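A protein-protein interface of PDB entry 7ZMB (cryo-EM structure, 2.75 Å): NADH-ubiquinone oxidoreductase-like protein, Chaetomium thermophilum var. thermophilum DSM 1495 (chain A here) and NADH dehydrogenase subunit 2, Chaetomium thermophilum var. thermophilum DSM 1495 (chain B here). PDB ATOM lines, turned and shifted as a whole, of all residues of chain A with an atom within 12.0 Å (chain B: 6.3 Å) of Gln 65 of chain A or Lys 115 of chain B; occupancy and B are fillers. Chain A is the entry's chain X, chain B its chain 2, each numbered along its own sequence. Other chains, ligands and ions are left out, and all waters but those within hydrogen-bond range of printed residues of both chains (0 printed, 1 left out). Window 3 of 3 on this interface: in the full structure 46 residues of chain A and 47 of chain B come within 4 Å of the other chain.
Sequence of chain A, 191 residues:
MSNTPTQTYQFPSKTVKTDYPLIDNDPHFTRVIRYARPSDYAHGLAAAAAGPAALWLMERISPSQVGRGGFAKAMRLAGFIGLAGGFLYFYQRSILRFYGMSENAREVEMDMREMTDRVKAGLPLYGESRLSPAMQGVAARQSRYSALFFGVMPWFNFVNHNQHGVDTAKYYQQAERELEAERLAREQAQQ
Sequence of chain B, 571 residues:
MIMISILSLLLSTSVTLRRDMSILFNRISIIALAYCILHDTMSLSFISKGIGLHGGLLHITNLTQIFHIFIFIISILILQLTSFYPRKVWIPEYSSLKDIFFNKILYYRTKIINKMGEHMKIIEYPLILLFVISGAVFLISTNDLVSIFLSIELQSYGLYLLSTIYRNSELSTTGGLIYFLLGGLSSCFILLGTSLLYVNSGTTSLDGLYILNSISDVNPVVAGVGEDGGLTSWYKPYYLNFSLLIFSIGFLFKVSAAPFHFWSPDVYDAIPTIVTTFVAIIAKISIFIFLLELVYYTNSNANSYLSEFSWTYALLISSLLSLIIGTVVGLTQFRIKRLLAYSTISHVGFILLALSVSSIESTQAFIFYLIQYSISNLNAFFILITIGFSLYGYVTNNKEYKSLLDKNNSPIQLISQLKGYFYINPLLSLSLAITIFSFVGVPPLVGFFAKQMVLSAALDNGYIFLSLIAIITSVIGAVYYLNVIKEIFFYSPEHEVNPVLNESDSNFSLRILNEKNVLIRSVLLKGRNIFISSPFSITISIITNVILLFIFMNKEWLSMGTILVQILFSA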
ATOM      1  N   LEU A  55      -7.669 -20.542   4.505  1.00  0.00           N
ATOM      2  CA  LEU A  55      -8.672 -20.241   3.489  1.00  0.00           C
ATOM      3  C   LEU A  55      -8.412 -18.899   2.822  1.00  0.00           C
ATOM      4  O   LEU A  55      -8.789 -18.700   1.666  1.00  0.00           O
ATOM      5  CB  LEU A  55     -10.073 -20.275   4.105  1.00  0.00           C
ATOM      6  CG  LEU A  55     -11.296 -20.236   3.176  1.00  0.00           C
ATOM      7  CD1 LEU A  55     -11.468 -21.527   2.400  1.00  0.00           C
ATOM      8  CD2 LEU A  55     -12.558 -19.920   3.943  1.00  0.00           C
ATOM      9  N   TRP A  56      -7.726 -17.987   3.502  1.00  0.00           N
ATOM     10  CA  TRP A  56      -7.307 -16.695   2.886  1.00  0.00           C
ATOM     11  C   TRP A  56      -6.226 -16.939   1.831  1.00  0.00           C
ATOM     12  O   TRP A  56      -6.338 -16.370   0.747  1.00  0.00           O
ATOM     13  CB  TRP A  56      -6.849 -15.662   3.917  1.00  0.00           C
ATOM     14  CG  TRP A  56      -6.639 -14.310   3.312  1.00  0.00           C
ATOM     15  CD1 TRP A  56      -7.578 -13.335   3.137  1.00  0.00           C
ATOM     16  CD2 TRP A  56      -5.413 -13.786   2.769  1.00  0.00           C
ATOM     17  NE1 TRP A  56      -7.020 -12.240   2.535  1.00  0.00           N
ATOM     18  CE2 TRP A  56      -5.694 -12.489   2.295  1.00  0.00           C
ATOM     19  CE3 TRP A  56      -4.113 -14.284   2.637  1.00  0.00           C
ATOM     20  CZ2 TRP A  56      -4.720 -11.687   1.702  1.00  0.00           C
ATOM     21  CZ3 TRP A  56      -3.153 -13.493   2.049  1.00  0.00           C
ATOM     22  CH2 TRP A  56      -3.453 -12.212   1.591  1.00  0.00           C
ATOM     23  N   LEU A  57      -5.189 -17.689   2.176  1.00  0.00           N
ATOM     24  CA  LEU A  57      -4.079 -17.969   1.247  1.00  0.00           C
ATOM     25  C   LEU A  57      -4.617 -18.734   0.031  1.00  0.00           C
ATOM     26  O   LEU A  57      -4.202 -18.421  -1.087  1.00  0.00           O
ATOM     27  CB  LEU A  57      -3.030 -18.773   2.025  1.00  0.00           C
ATOM     28  CG  LEU A  57      -1.767 -19.152   1.260  1.00  0.00           C
ATOM     29  CD1 LEU A  57      -1.109 -17.910   0.691  1.00  0.00           C
ATOM     30  CD2 LEU A  57      -0.798 -19.894   2.164  1.00  0.00           C
ATOM     31  N   MET A  58      -5.517 -19.690   0.242  1.00  0.00           N
ATOM     32  CA  MET A  58      -6.103 -20.456  -0.886  1.00  0.00           C
ATOM     33  C   MET A  58      -6.862 -19.479  -1.775  1.00  0.00           C
ATOM     34  O   MET A  58      -6.808 -19.642  -2.996  1.00  0.00           O
ATOM     35  CB  MET A  58      -7.030 -21.580  -0.416  1.00  0.00           C
ATOM     36  CG  MET A  58      -6.294 -22.850  -0.038  1.00  0.00           C
ATOM     37  SD  MET A  58      -7.388 -24.181   0.519  1.00  0.00           S
ATOM     38  CE  MET A  58      -7.774 -23.635   2.179  1.00  0.00           C
ATOM     39  N   GLU A  59      -7.556 -18.520  -1.172  1.00  0.00           N
ATOM     40  CA  GLU A  59      -8.255 -17.479  -1.964  1.00  0.00           C
ATOM     41  C   GLU A  59      -7.235 -16.629  -2.710  1.00  0.00           C
ATOM     42  O   GLU A  59      -7.493 -16.312  -3.880  1.00  0.00           O
ATOM     43  CB  GLU A  59      -9.112 -16.593  -1.064  1.00  0.00           C
ATOM     44  CG  GLU A  59     -10.131 -15.773  -1.837  1.00  0.00           C
ATOM     45  CD  GLU A  59     -11.118 -16.585  -2.658  1.00  0.00           C
ATOM     46  OE1 GLU A  59     -11.457 -17.708  -2.242  1.00  0.00           O
ATOM     47  OE2 GLU A  59     -11.544 -16.092  -3.716  1.00  0.00           O
ATOM     48  N   ARG A  60      -6.142 -16.234  -2.059  1.00  0.00           N
ATOM     49  CA  ARG A  60      -5.212 -15.319  -2.764  1.00  0.00           C
ATOM     50  C   ARG A  60      -4.529 -16.041  -3.926  1.00  0.00           C
ATOM     51  O   ARG A  60      -4.490 -15.475  -5.032  1.00  0.00           O
ATOM     52  CB  ARG A  60      -4.205 -14.702  -1.791  1.00  0.00           C
ATOM     53  CG  ARG A  60      -3.504 -13.467  -2.335  1.00  0.00           C
ATOM     54  CD  ARG A  60      -4.513 -12.362  -2.571  1.00  0.00           C
ATOM     55  NE  ARG A  60      -3.948 -11.228  -3.283  1.00  0.00           N
ATOM     56  CZ  ARG A  60      -3.388 -10.177  -2.699  1.00  0.00           C
ATOM     57  NH1 ARG A  60      -3.312 -10.113  -1.381  1.00  0.00           N
ATOM     58  NH2 ARG A  60      -2.901  -9.194  -3.435  1.00  0.00           N
ATOM     59  N   ILE A  61      -4.000 -17.235  -3.677  1.00  0.00           N
ATOM     60  CA  ILE A  61      -3.243 -17.962  -4.734  1.00  0.00           C
ATOM     61  C   ILE A  61      -4.201 -18.516  -5.793  1.00  0.00           C
ATOM     62  O   ILE A  61      -3.873 -18.426  -6.986  1.00  0.00           O
ATOM     63  CB  ILE A  61      -2.331 -19.035  -4.106  1.00  0.00           C
ATOM     64  CG1 ILE A  61      -1.394 -18.436  -3.057  1.00  0.00           C
ATOM     65  CG2 ILE A  61      -1.560 -19.792  -5.176  1.00  0.00           C
ATOM     66  CD1 ILE A  61      -0.410 -19.427  -2.494  1.00  0.00           C
ATOM     67  N   SER A  62      -5.336 -19.073  -5.371  1.00  0.00           N
ATOM     68  CA  SER A  62      -6.265 -19.741  -6.324  1.00  0.00           C
ATOM     69  C   SER A  62      -7.701 -19.285  -6.065  1.00  0.00           C
ATOM     70  O   SER A  62      -8.438 -20.022  -5.431  1.00  0.00           O
ATOM     71  CB  SER A  62      -6.112 -21.236  -6.249  1.00  0.00           C
ATOM     72  OG  SER A  62      -6.175 -21.690  -4.908  1.00  0.00           O
ATOM     73  N   PRO A  63      -8.179 -18.096  -6.521  1.00  0.00           N
ATOM     74  CA  PRO A  63      -9.576 -17.722  -6.244  1.00  0.00           C
ATOM     75  C   PRO A  63     -10.727 -18.689  -6.556  1.00  0.00           C
ATOM     76  O   PRO A  63     -10.675 -19.361  -7.548  1.00  0.00           O
ATOM     77  CB  PRO A  63      -9.750 -16.428  -7.046  1.00  0.00           C
ATOM     78  CG  PRO A  63      -8.364 -15.853  -7.142  1.00  0.00           C
ATOM     79  CD  PRO A  63      -7.477 -17.063  -7.311  1.00  0.00           C
ATOM     80  N   SER A  64     -11.789 -18.633  -5.759  1.00  0.00           N
ATOM     81  CA  SER A  64     -12.955 -19.525  -5.946  1.00  0.00           C
ATOM     82  C   SER A  64     -13.892 -18.957  -7.014  1.00  0.00           C
ATOM     83  O   SER A  64     -14.775 -19.707  -7.445  1.00  0.00           O
ATOM     84  CB  SER A  64     -13.657 -19.650  -4.626  1.00  0.00           C
ATOM     85  OG  SER A  64     -13.684 -18.397  -3.964  1.00  0.00           O
ATOM     86  N   GLN A  65     -13.719 -17.685  -7.393  1.00  0.00           N
ATOM     87  CA  GLN A  65     -14.613 -16.994  -8.369  1.00  0.00           C
ATOM     88  C   GLN A  65     -16.026 -16.955  -7.792  1.00  0.00           C
ATOM     89  O   GLN A  65     -16.977 -17.029  -8.574  1.00  0.00           O
ATOM     90  CB  GLN A  65     -14.526 -17.634  -9.759  1.00  0.00           C
ATOM     91  CG  GLN A  65     -13.102 -17.857 -10.248  1.00  0.00           C
ATOM     92  CD  GLN A  65     -12.316 -16.577 -10.368  1.00  0.00           C
ATOM     93  OE1 GLN A  65     -11.170 -16.490  -9.937  1.00  0.00           O
ATOM     94  NE2 GLN A  65     -12.929 -15.566 -10.963  1.00  0.00           N
ATOM     95  N   VAL A  66     -16.140 -16.828  -6.470  1.00  0.00           N
ATOM     96  CA  VAL A  66     -17.460 -16.807  -5.775  1.00  0.00           C
ATOM     97  C   VAL A  66     -18.135 -15.456  -6.009  1.00  0.00           C
ATOM     98  O   VAL A  66     -17.438 -14.522  -6.435  1.00  0.00           O
ATOM     99  CB  VAL A  66     -17.290 -17.137  -4.277  1.00  0.00           C
ATOM    100  CG1 VAL A  66     -16.557 -16.048  -3.516  1.00  0.00           C
ATOM    101  CG2 VAL A  66     -18.597 -17.507  -3.593  1.00  0.00           C
ATOM    102  N   GLY A  67     -19.446 -15.370  -5.772  1.00  0.00           N
ATOM    103  CA  GLY A  67     -20.188 -14.105  -5.899  1.00  0.00           C
ATOM    104  C   GLY A  67     -19.696 -12.987  -5.004  1.00  0.00           C
ATOM    105  O   GLY A  67     -18.578 -13.072  -4.519  1.00  0.00           O
ATOM    106  N   ARG A  68     -20.528 -11.990  -4.734  1.00  0.00           N
ATOM    107  CA  ARG A  68     -20.119 -10.788  -4.011  1.00  0.00           C
ATOM    108  C   ARG A  68     -20.041 -10.957  -2.500  1.00  0.00           C
ATOM    109  O   ARG A  68     -19.304 -10.208  -1.853  1.00  0.00           O
ATOM    110  CB  ARG A  68     -21.077  -9.640  -4.319  1.00  0.00           C
ATOM    111  CG  ARG A  68     -21.100  -9.200  -5.771  1.00  0.00           C
ATOM    112  CD  ARG A  68     -21.774  -7.847  -5.932  1.00  0.00           C
ATOM    113  NE  ARG A  68     -22.149  -7.583  -7.318  1.00  0.00           N
ATOM    114  CZ  ARG A  68     -21.301  -7.183  -8.261  1.00  0.00           C
ATOM    115  NH1 ARG A  68     -20.022  -6.994  -7.970  1.00  0.00           N
ATOM    116  NH2 ARG A  68     -21.734  -6.969  -9.496  1.00  0.00           N
ATOM    117  N   GLY A  69     -20.780 -11.890  -1.912  1.00  0.00           N
ATOM    118  CA  GLY A  69     -20.748 -11.989  -0.466  1.00  0.00           C
ATOM    119  C   GLY A  69     -20.496 -13.382   0.065  1.00  0.00           C
ATOM    120  O   GLY A  69     -20.736 -13.664   1.242  1.00  0.00           O
ATOM    121  N   GLY A  70     -20.002 -14.264  -0.806  1.00  0.00           N
ATOM    122  CA  GLY A  70     -19.795 -15.644  -0.417  1.00  0.00           C
ATOM    123  C   GLY A  70     -18.535 -15.885   0.378  1.00  0.00           C
ATOM    124  O   GLY A  70     -18.516 -16.757   1.250  1.00  0.00           O
ATOM    125  N   PHE A  71     -17.466 -15.137   0.095  1.00  0.00           N
ATOM    126  CA  PHE A  71     -16.215 -15.389   0.801  1.00  0.00           C
ATOM    127  C   PHE A  71     -16.298 -14.945   2.253  1.00  0.00           C
ATOM    128  O   PHE A  71     -15.768 -15.620   3.141  1.00  0.00           O
ATOM    129  CB  PHE A  71     -15.037 -14.708   0.112  1.00  0.00           C
ATOM    130  CG  PHE A  71     -13.728 -15.025   0.755  1.00  0.00           C
ATOM    131  CD1 PHE A  71     -13.116 -16.244   0.532  1.00  0.00           C
ATOM    132  CD2 PHE A  71     -13.137 -14.137   1.635  1.00  0.00           C
ATOM    133  CE1 PHE A  71     -11.929 -16.559   1.151  1.00  0.00           C
ATOM    134  CE2 PHE A  71     -11.947 -14.455   2.256  1.00  0.00           C
ATOM    135  CZ  PHE A  71     -11.344 -15.661   2.009  1.00  0.00           C
ATOM    136  N   ALA A  72     -16.961 -13.818   2.514  1.00  0.00           N
ATOM    137  CA  ALA A  72     -17.181 -13.392   3.890  1.00  0.00           C
ATOM    138  C   ALA A  72     -17.990 -14.426   4.658  1.00  0.00           C
ATOM    139  O   ALA A  72     -17.749 -14.656   5.847  1.00  0.00           O
ATOM    140  CB  ALA A  72     -17.881 -12.033   3.912  1.00  0.00           C
ATOM    141  N   ALA A  74     -17.847 -17.675   4.015  1.00  0.00           N
ATOM    142  CA  ALA A  74     -16.938 -18.794   4.239  1.00  0.00           C
ATOM    143  C   ALA A  74     -15.919 -18.483   5.327  1.00  0.00           C
ATOM    144  O   ALA A  74     -15.479 -19.391   6.038  1.00  0.00           O
ATOM    145  CB  ALA A  74     -16.229 -19.166   2.938  1.00  0.00           C
ATOM    146  N   ASP B  20     -22.517 -21.526  -5.986  1.00  0.00           N
ATOM    147  CA  ASP B  20     -21.137 -20.990  -6.092  1.00  0.00           C
ATOM    148  C   ASP B  20     -20.364 -21.258  -4.793  1.00  0.00           C
ATOM    149  O   ASP B  20     -19.132 -21.119  -4.808  1.00  0.00           O
ATOM    150  CB  ASP B  20     -21.166 -19.508  -6.479  1.00  0.00           C
ATOM    151  CG  ASP B  20     -21.928 -18.587  -5.547  1.00  0.00           C
ATOM    152  OD1 ASP B  20     -22.533 -19.087  -4.591  1.00  0.00           O
ATOM    153  OD2 ASP B  20     -21.898 -17.370  -5.790  1.00  0.00           O
ATOM    154  N   ILE B  23     -17.395 -24.839  -3.861  1.00  0.00           N
ATOM    155  CA  ILE B  23     -15.904 -24.837  -3.856  1.00  0.00           C
ATOM    156  C   ILE B  23     -15.382 -24.393  -2.485  1.00  0.00           C
ATOM    157  O   ILE B  23     -14.400 -24.996  -2.026  1.00  0.00           O
ATOM    158  CB  ILE B  23     -15.341 -23.988  -5.014  1.00  0.00           C
ATOM    159  CG1 ILE B  23     -13.813 -24.011  -5.069  1.00  0.00           C
ATOM    160  CG2 ILE B  23     -15.887 -22.568  -4.984  1.00  0.00           C
ATOM    161  CD1 ILE B  23     -13.260 -24.290  -6.442  1.00  0.00           C
ATOM    162  N   TYR B  85     -10.171 -25.800  -9.041  1.00  0.00           N
ATOM    163  CA  TYR B  85     -10.622 -25.976 -10.442  1.00  0.00           C
ATOM    164  C   TYR B  85      -9.651 -26.906 -11.169  1.00  0.00           C
ATOM    165  O   TYR B  85      -8.459 -26.880 -10.858  1.00  0.00           O
ATOM    166  CB  TYR B  85     -10.865 -24.621 -11.108  1.00  0.00           C
ATOM    167  CG  TYR B  85     -12.056 -23.884 -10.558  1.00  0.00           C
ATOM    168  CD1 TYR B  85     -13.344 -24.312 -10.828  1.00  0.00           C
ATOM    169  CD2 TYR B  85     -11.898 -22.767  -9.757  1.00  0.00           C
ATOM    170  CE1 TYR B  85     -14.445 -23.648 -10.319  1.00  0.00           C
ATOM    171  CE2 TYR B  85     -12.987 -22.088  -9.244  1.00  0.00           C
ATOM    172  CZ  TYR B  85     -14.265 -22.530  -9.527  1.00  0.00           C
ATOM    173  OH  TYR B  85     -15.344 -21.868  -9.023  1.00  0.00           O
ATOM    174  N   TYR B 107      -9.095 -12.482 -16.423  1.00  0.00           N
ATOM    175  CA  TYR B 107      -9.397 -13.063 -17.724  1.00  0.00           C
ATOM    176  C   TYR B 107     -10.696 -13.840 -17.605  1.00  0.00           C
ATOM    177  O   TYR B 107     -11.153 -14.145 -16.504  1.00  0.00           O
ATOM    178  CB  TYR B 107      -8.258 -13.959 -18.224  1.00  0.00           C
ATOM    179  CG  TYR B 107      -8.073 -15.256 -17.465  1.00  0.00           C
ATOM    180  CD1 TYR B 107      -7.489 -15.275 -16.205  1.00  0.00           C
ATOM    181  CD2 TYR B 107      -8.479 -16.460 -18.015  1.00  0.00           C
ATOM    182  CE1 TYR B 107      -7.320 -16.453 -15.527  1.00  0.00           C
ATOM    183  CE2 TYR B 107      -8.317 -17.634 -17.341  1.00  0.00           C
ATOM    184  CZ  TYR B 107      -7.738 -17.632 -16.101  1.00  0.00           C
ATOM    185  OH  TYR B 107      -7.580 -18.823 -15.441  1.00  0.00           O
ATOM    186  N   TYR B 108     -11.289 -14.156 -18.749  1.00  0.00           N
ATOM    187  CA  TYR B 108     -12.503 -14.968 -18.773  1.00  0.00           C
ATOM    188  C   TYR B 108     -12.127 -16.408 -18.446  1.00  0.00           C
ATOM    189  O   TYR B 108     -11.623 -17.140 -19.301  1.00  0.00           O
ATOM    190  CB  TYR B 108     -13.191 -14.874 -20.130  1.00  0.00           C
ATOM    191  CG  TYR B 108     -14.550 -15.530 -20.138  1.00  0.00           C
ATOM    192  CD1 TYR B 108     -15.444 -15.321 -19.100  1.00  0.00           C
ATOM    193  CD2 TYR B 108     -14.914 -16.409 -21.143  1.00  0.00           C
ATOM    194  CE1 TYR B 108     -16.675 -15.932 -19.088  1.00  0.00           C
ATOM    195  CE2 TYR B 108     -16.142 -17.036 -21.128  1.00  0.00           C
ATOM    196  CZ  TYR B 108     -17.015 -16.796 -20.097  1.00  0.00           C
ATOM    197  OH  TYR B 108     -18.245 -17.404 -20.079  1.00  0.00           O
ATOM    198  N   ARG B 109     -12.453 -16.863 -17.241  1.00  0.00           N
ATOM    199  CA  ARG B 109     -12.050 -18.237 -16.844  1.00  0.00           C
ATOM    200  C   ARG B 109     -13.257 -19.170 -16.802  1.00  0.00           C
ATOM    201  O   ARG B 109     -13.033 -20.352 -16.557  1.00  0.00           O
ATOM    202  CB  ARG B 109     -11.446 -18.266 -15.440  1.00  0.00           C
ATOM    203  CG  ARG B 109     -11.046 -16.931 -14.839  1.00  0.00           C
ATOM    204  CD  ARG B 109     -10.300 -17.226 -13.551  1.00  0.00           C
ATOM    205  NE  ARG B 109      -9.504 -16.109 -13.069  1.00  0.00           N
ATOM    206  CZ  ARG B 109      -8.549 -16.199 -12.153  1.00  0.00           C
ATOM    207  NH1 ARG B 109      -8.252 -17.370 -11.617  1.00  0.00           N
ATOM    208  NH2 ARG B 109      -7.882 -15.122 -11.787  1.00  0.00           N
ATOM    209  N   THR B 110     -14.465 -18.700 -17.132  1.00  0.00           N
ATOM    210  CA  THR B 110     -15.660 -19.555 -16.895  1.00  0.00           C
ATOM    211  C   THR B 110     -15.552 -20.874 -17.655  1.00  0.00           C
ATOM    212  O   THR B 110     -15.829 -21.919 -17.039  1.00  0.00           O
ATOM    213  CB  THR B 110     -16.984 -18.814 -17.112  1.00  0.00           C
ATOM    214  OG1 THR B 110     -16.912 -17.606 -16.357  1.00  0.00           O
ATOM    215  CG2 THR B 110     -18.192 -19.610 -16.675  1.00  0.00           C
ATOM    216  N   LYS B 111     -15.115 -20.834 -18.914  1.00  0.00           N
ATOM    217  CA  LYS B 111     -15.047 -22.083 -19.708  1.00  0.00           C
ATOM    218  C   LYS B 111     -13.732 -22.814 -19.416  1.00  0.00           C
ATOM    219  O   LYS B 111     -13.796 -24.037 -19.247  1.00  0.00           O
ATOM    220  CB  LYS B 111     -15.264 -21.759 -21.185  1.00  0.00           C
ATOM    221  CG  LYS B 111     -16.518 -20.948 -21.473  1.00  0.00           C
ATOM    222  CD  LYS B 111     -16.781 -20.760 -22.943  1.00  0.00           C
ATOM    223  CE  LYS B 111     -18.226 -20.414 -23.219  1.00  0.00           C
ATOM    224  NZ  LYS B 111     -19.145 -21.336 -22.511  1.00  0.00           N
ATOM    225  N   ILE B 112     -12.604 -22.106 -19.285  1.00  0.00           N
ATOM    226  CA  ILE B 112     -11.299 -22.739 -19.117  1.00  0.00           C
ATOM    227  C   ILE B 112     -11.249 -23.538 -17.820  1.00  0.00           C
ATOM    228  O   ILE B 112     -10.749 -24.668 -17.787  1.00  0.00           O
ATOM    229  CB  ILE B 112     -10.181 -21.680 -19.170  1.00  0.00           C
ATOM    230  CG1 ILE B 112      -9.860 -21.303 -20.617  1.00  0.00           C
ATOM    231  CG2 ILE B 112      -8.931 -22.185 -18.487  1.00  0.00           C
ATOM    232  CD1 ILE B 112      -9.190 -19.983 -20.762  1.00  0.00           C
ATOM    233  N   ILE B 113     -11.829 -22.995 -16.746  1.00  0.00           N
ATOM    234  CA  ILE B 113     -11.750 -23.655 -15.406  1.00  0.00           C
ATOM    235  C   ILE B 113     -12.990 -24.522 -15.128  1.00  0.00           C
ATOM    236  O   ILE B 113     -13.018 -25.142 -14.058  1.00  0.00           O
ATOM    237  CB  ILE B 113     -11.510 -22.618 -14.292  1.00  0.00           C
ATOM    238  CG1 ILE B 113     -12.796 -21.884 -13.898  1.00  0.00           C
ATOM    239  CG2 ILE B 113     -10.385 -21.667 -14.671  1.00  0.00           C
ATOM    240  CD1 ILE B 113     -12.616 -20.847 -12.823  1.00  0.00           C
ATOM    241  N   ASN B 114     -13.958 -24.589 -16.053  1.00  0.00           N
ATOM    242  CA  ASN B 114     -15.244 -25.314 -15.820  1.00  0.00           C
ATOM    243  C   ASN B 114     -15.831 -24.877 -14.473  1.00  0.00           C
ATOM    244  O   ASN B 114     -16.172 -25.754 -13.659  1.00  0.00           O
ATOM    245  CB  ASN B 114     -15.143 -26.824 -16.020  1.00  0.00           C
ATOM    246  CG  ASN B 114     -16.486 -27.481 -16.263  1.00  0.00           C
ATOM    247  OD1 ASN B 114     -17.486 -26.800 -16.467  1.00  0.00           O
ATOM    248  ND2 ASN B 114     -16.517 -28.802 -16.244  1.00  0.00           N
ATOM    249  N   LYS B 115     -15.978 -23.568 -14.273  1.00  0.00           N
ATOM    250  CA  LYS B 115     -16.498 -23.003 -13.003  1.00  0.00           C
ATOM    251  C   LYS B 115     -17.862 -23.595 -12.670  1.00  0.00           C
ATOM    252  O   LYS B 115     -18.104 -23.875 -11.483  1.00  0.00           O
ATOM    253  CB  LYS B 115     -16.596 -21.481 -13.144  1.00  0.00           C
ATOM    254  CG  LYS B 115     -17.128 -20.711 -11.948  1.00  0.00           C
ATOM    255  CD  LYS B 115     -17.326 -19.250 -12.276  1.00  0.00           C
ATOM    256  CE  LYS B 115     -16.170 -18.670 -13.061  1.00  0.00           C
ATOM    257  NZ  LYS B 115     -16.308 -17.208 -13.256  1.00  0.00           N
ATOM    258  N   MET B 116     -18.695 -23.822 -13.680  1.00  0.00           N
ATOM    259  CA  MET B 116     -20.090 -24.277 -13.449  1.00  0.00           C
ATOM    260  C   MET B 116     -20.220 -25.781 -13.702  1.00  0.00           C
ATOM    261  O   MET B 116     -21.338 -26.220 -13.983  1.00  0.00           O
ATOM    262  CB  MET B 116     -21.059 -23.472 -14.314  1.00  0.00           C
ATOM    263  CG  MET B 116     -20.688 -22.009 -14.361  1.00  0.00           C
ATOM    264  SD  MET B 116     -22.093 -20.885 -14.284  1.00  0.00           S
ATOM    265  CE  MET B 116     -21.231 -19.340 -14.014  1.00  0.00           C
ATOM    266  N   GLY B 117     -19.133 -26.545 -13.553  1.00  0.00           N
ATOM    267  CA  GLY B 117     -19.197 -28.012 -13.699  1.00  0.00           C
ATOM    268  C   GLY B 117     -19.971 -28.668 -12.570  1.00  0.00           C
ATOM    269  O   GLY B 117     -20.118 -28.033 -11.517  1.00  0.00           O
ATOM    270  N   MET B 120     -18.424 -28.982  -9.167  1.00  0.00           N
ATOM    271  CA  MET B 120     -18.293 -27.668  -8.483  1.00  0.00           C
ATOM    272  C   MET B 120     -19.647 -27.097  -8.049  1.00  0.00           C
ATOM    273  O   MET B 120     -19.657 -25.965  -7.570  1.00  0.00           O
ATOM    274  CB  MET B 120     -17.603 -26.664  -9.410  1.00  0.00           C
ATOM    275  CG  MET B 120     -16.231 -27.112  -9.862  1.00  0.00           C
ATOM    276  SD  MET B 120     -15.078 -27.350  -8.482  1.00  0.00           S
ATOM    277  CE  MET B 120     -13.635 -27.894  -9.387  1.00  0.00           C
ATOM    278  N   LYS B 121     -20.754 -27.819  -8.226  1.00  0.00           N
ATOM    279  CA  LYS B 121     -22.073 -27.195  -7.930  1.00  0.00           C
ATOM    280  C   LYS B 121     -22.891 -27.962  -6.881  1.00  0.00           C
ATOM    281  O   LYS B 121     -23.999 -27.493  -6.576  1.00  0.00           O
ATOM    282  CB  LYS B 121     -22.874 -27.019  -9.222  1.00  0.00           C
ATOM    283  CG  LYS B 121     -22.391 -25.921 -10.158  1.00  0.00           C
ATOM    284  CD  LYS B 121     -23.396 -25.601 -11.239  1.00  0.00           C
ATOM    285  CE  LYS B 121     -23.865 -26.826 -11.993  1.00  0.00           C
ATOM    286  NZ  LYS B 121     -24.719 -26.460 -13.146  1.00  0.00           N
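Of chain B, only Arg 109 (3.4 Å), Ile 113 (3.98 Å) and Lys 115 (3.8 Å) come within 4 Å of Gln 65 of chain A.
Lys 115 of chain B touches one residue of chain A.
Of chain A, only Gln 65 comes within 4 Å of Arg 109 of chain B.
No residue of chain A comes within 4 Å of Thr 110 of chain B.
Of chain A, only Gln 65 comes within 4 Å of Ile 113 of chain B.
No residue of chain A comes within 4 Å of Asn 114 of chain B.
Printed residues of chain B within 4 Å of Ser 64 of chain A: Ile 23 (3.7 Å) and Tyr 85 (2.7 Å).
Printed residues of chain B within 4 Å of Val 66 of chain A: Asp 20.
Printed residues of chain A within 4 Å of Tyr 85 of chain B: Pro 63 (3.96 Å) and Ser 64 (2.7 Å).
Of the printed residues of chain B, Gly 67 of chain A touches Asp 20 (3.2 Å).
Of the printed residues of chain B, Pro 63 of chain A touches Tyr 85.
Ile 61 of chain A touches none of the printed residues of chain B.
The nearest residue of chain A that does not touch Lys 115 of chain B is Ser 64 of chain A (5.2 Å).
The nearest printed residue of chain B that does not touch Gly 67 of chain A is Lys 115 of chain B (7.9 Å).
Among the printed residues, merely in contact across the chains: Pro 63 of chain A with Tyr 85 of chain B (3.96 Å), Ser 64 of chain A with Ile 23 of chain B (3.7 Å), Gln 65 of chain A with Ile 113 of chain B (3.98 Å), Gln 65 of chain A with Lys 115 of chain B (3.8 Å) and Val 66 of chain A with Asp 20 of chain B (3.8 Å).
Of the 16 printed residues of chain B, 6 touch a printed residue of chain A.
Hydrophobic or aromatic side chains of chain B that line the printed part of chain A: Ile 23, Tyr 85 and Ile 113.
Of the 19 printed residues of chain A, 5 touch a printed residue of chain B.
Among the printed residues, no Asp or Glu carboxylate lies within 4 Å of a Lys or Arg side-chain nitrogen of the other chain.
O of Ser 64 of chain A lies within hydrogen-bond range of OH of Tyr 85 of chain B, 2.7 Å away.
NH1 of Arg 109 of chain B sits close to OE1 of Gln 65 of chain A (3.5 Å).
The backbone NH (N) of Gly 67 of chain A sits at hydrogen-bond distance from the side-chain carboxylate (OD2) of Asp 20 of chain B (3.2 Å).
The side-chain hydroxyl of Thr 110 of chain B is in hydrogen-bond range of the side-chain amino group of Lys 115 of chain B (3.2 Å).
OG of Ser 64 of chain A lies within hydrogen-bond range of OE1 of Glu 59 of chain A (2.9 Å).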
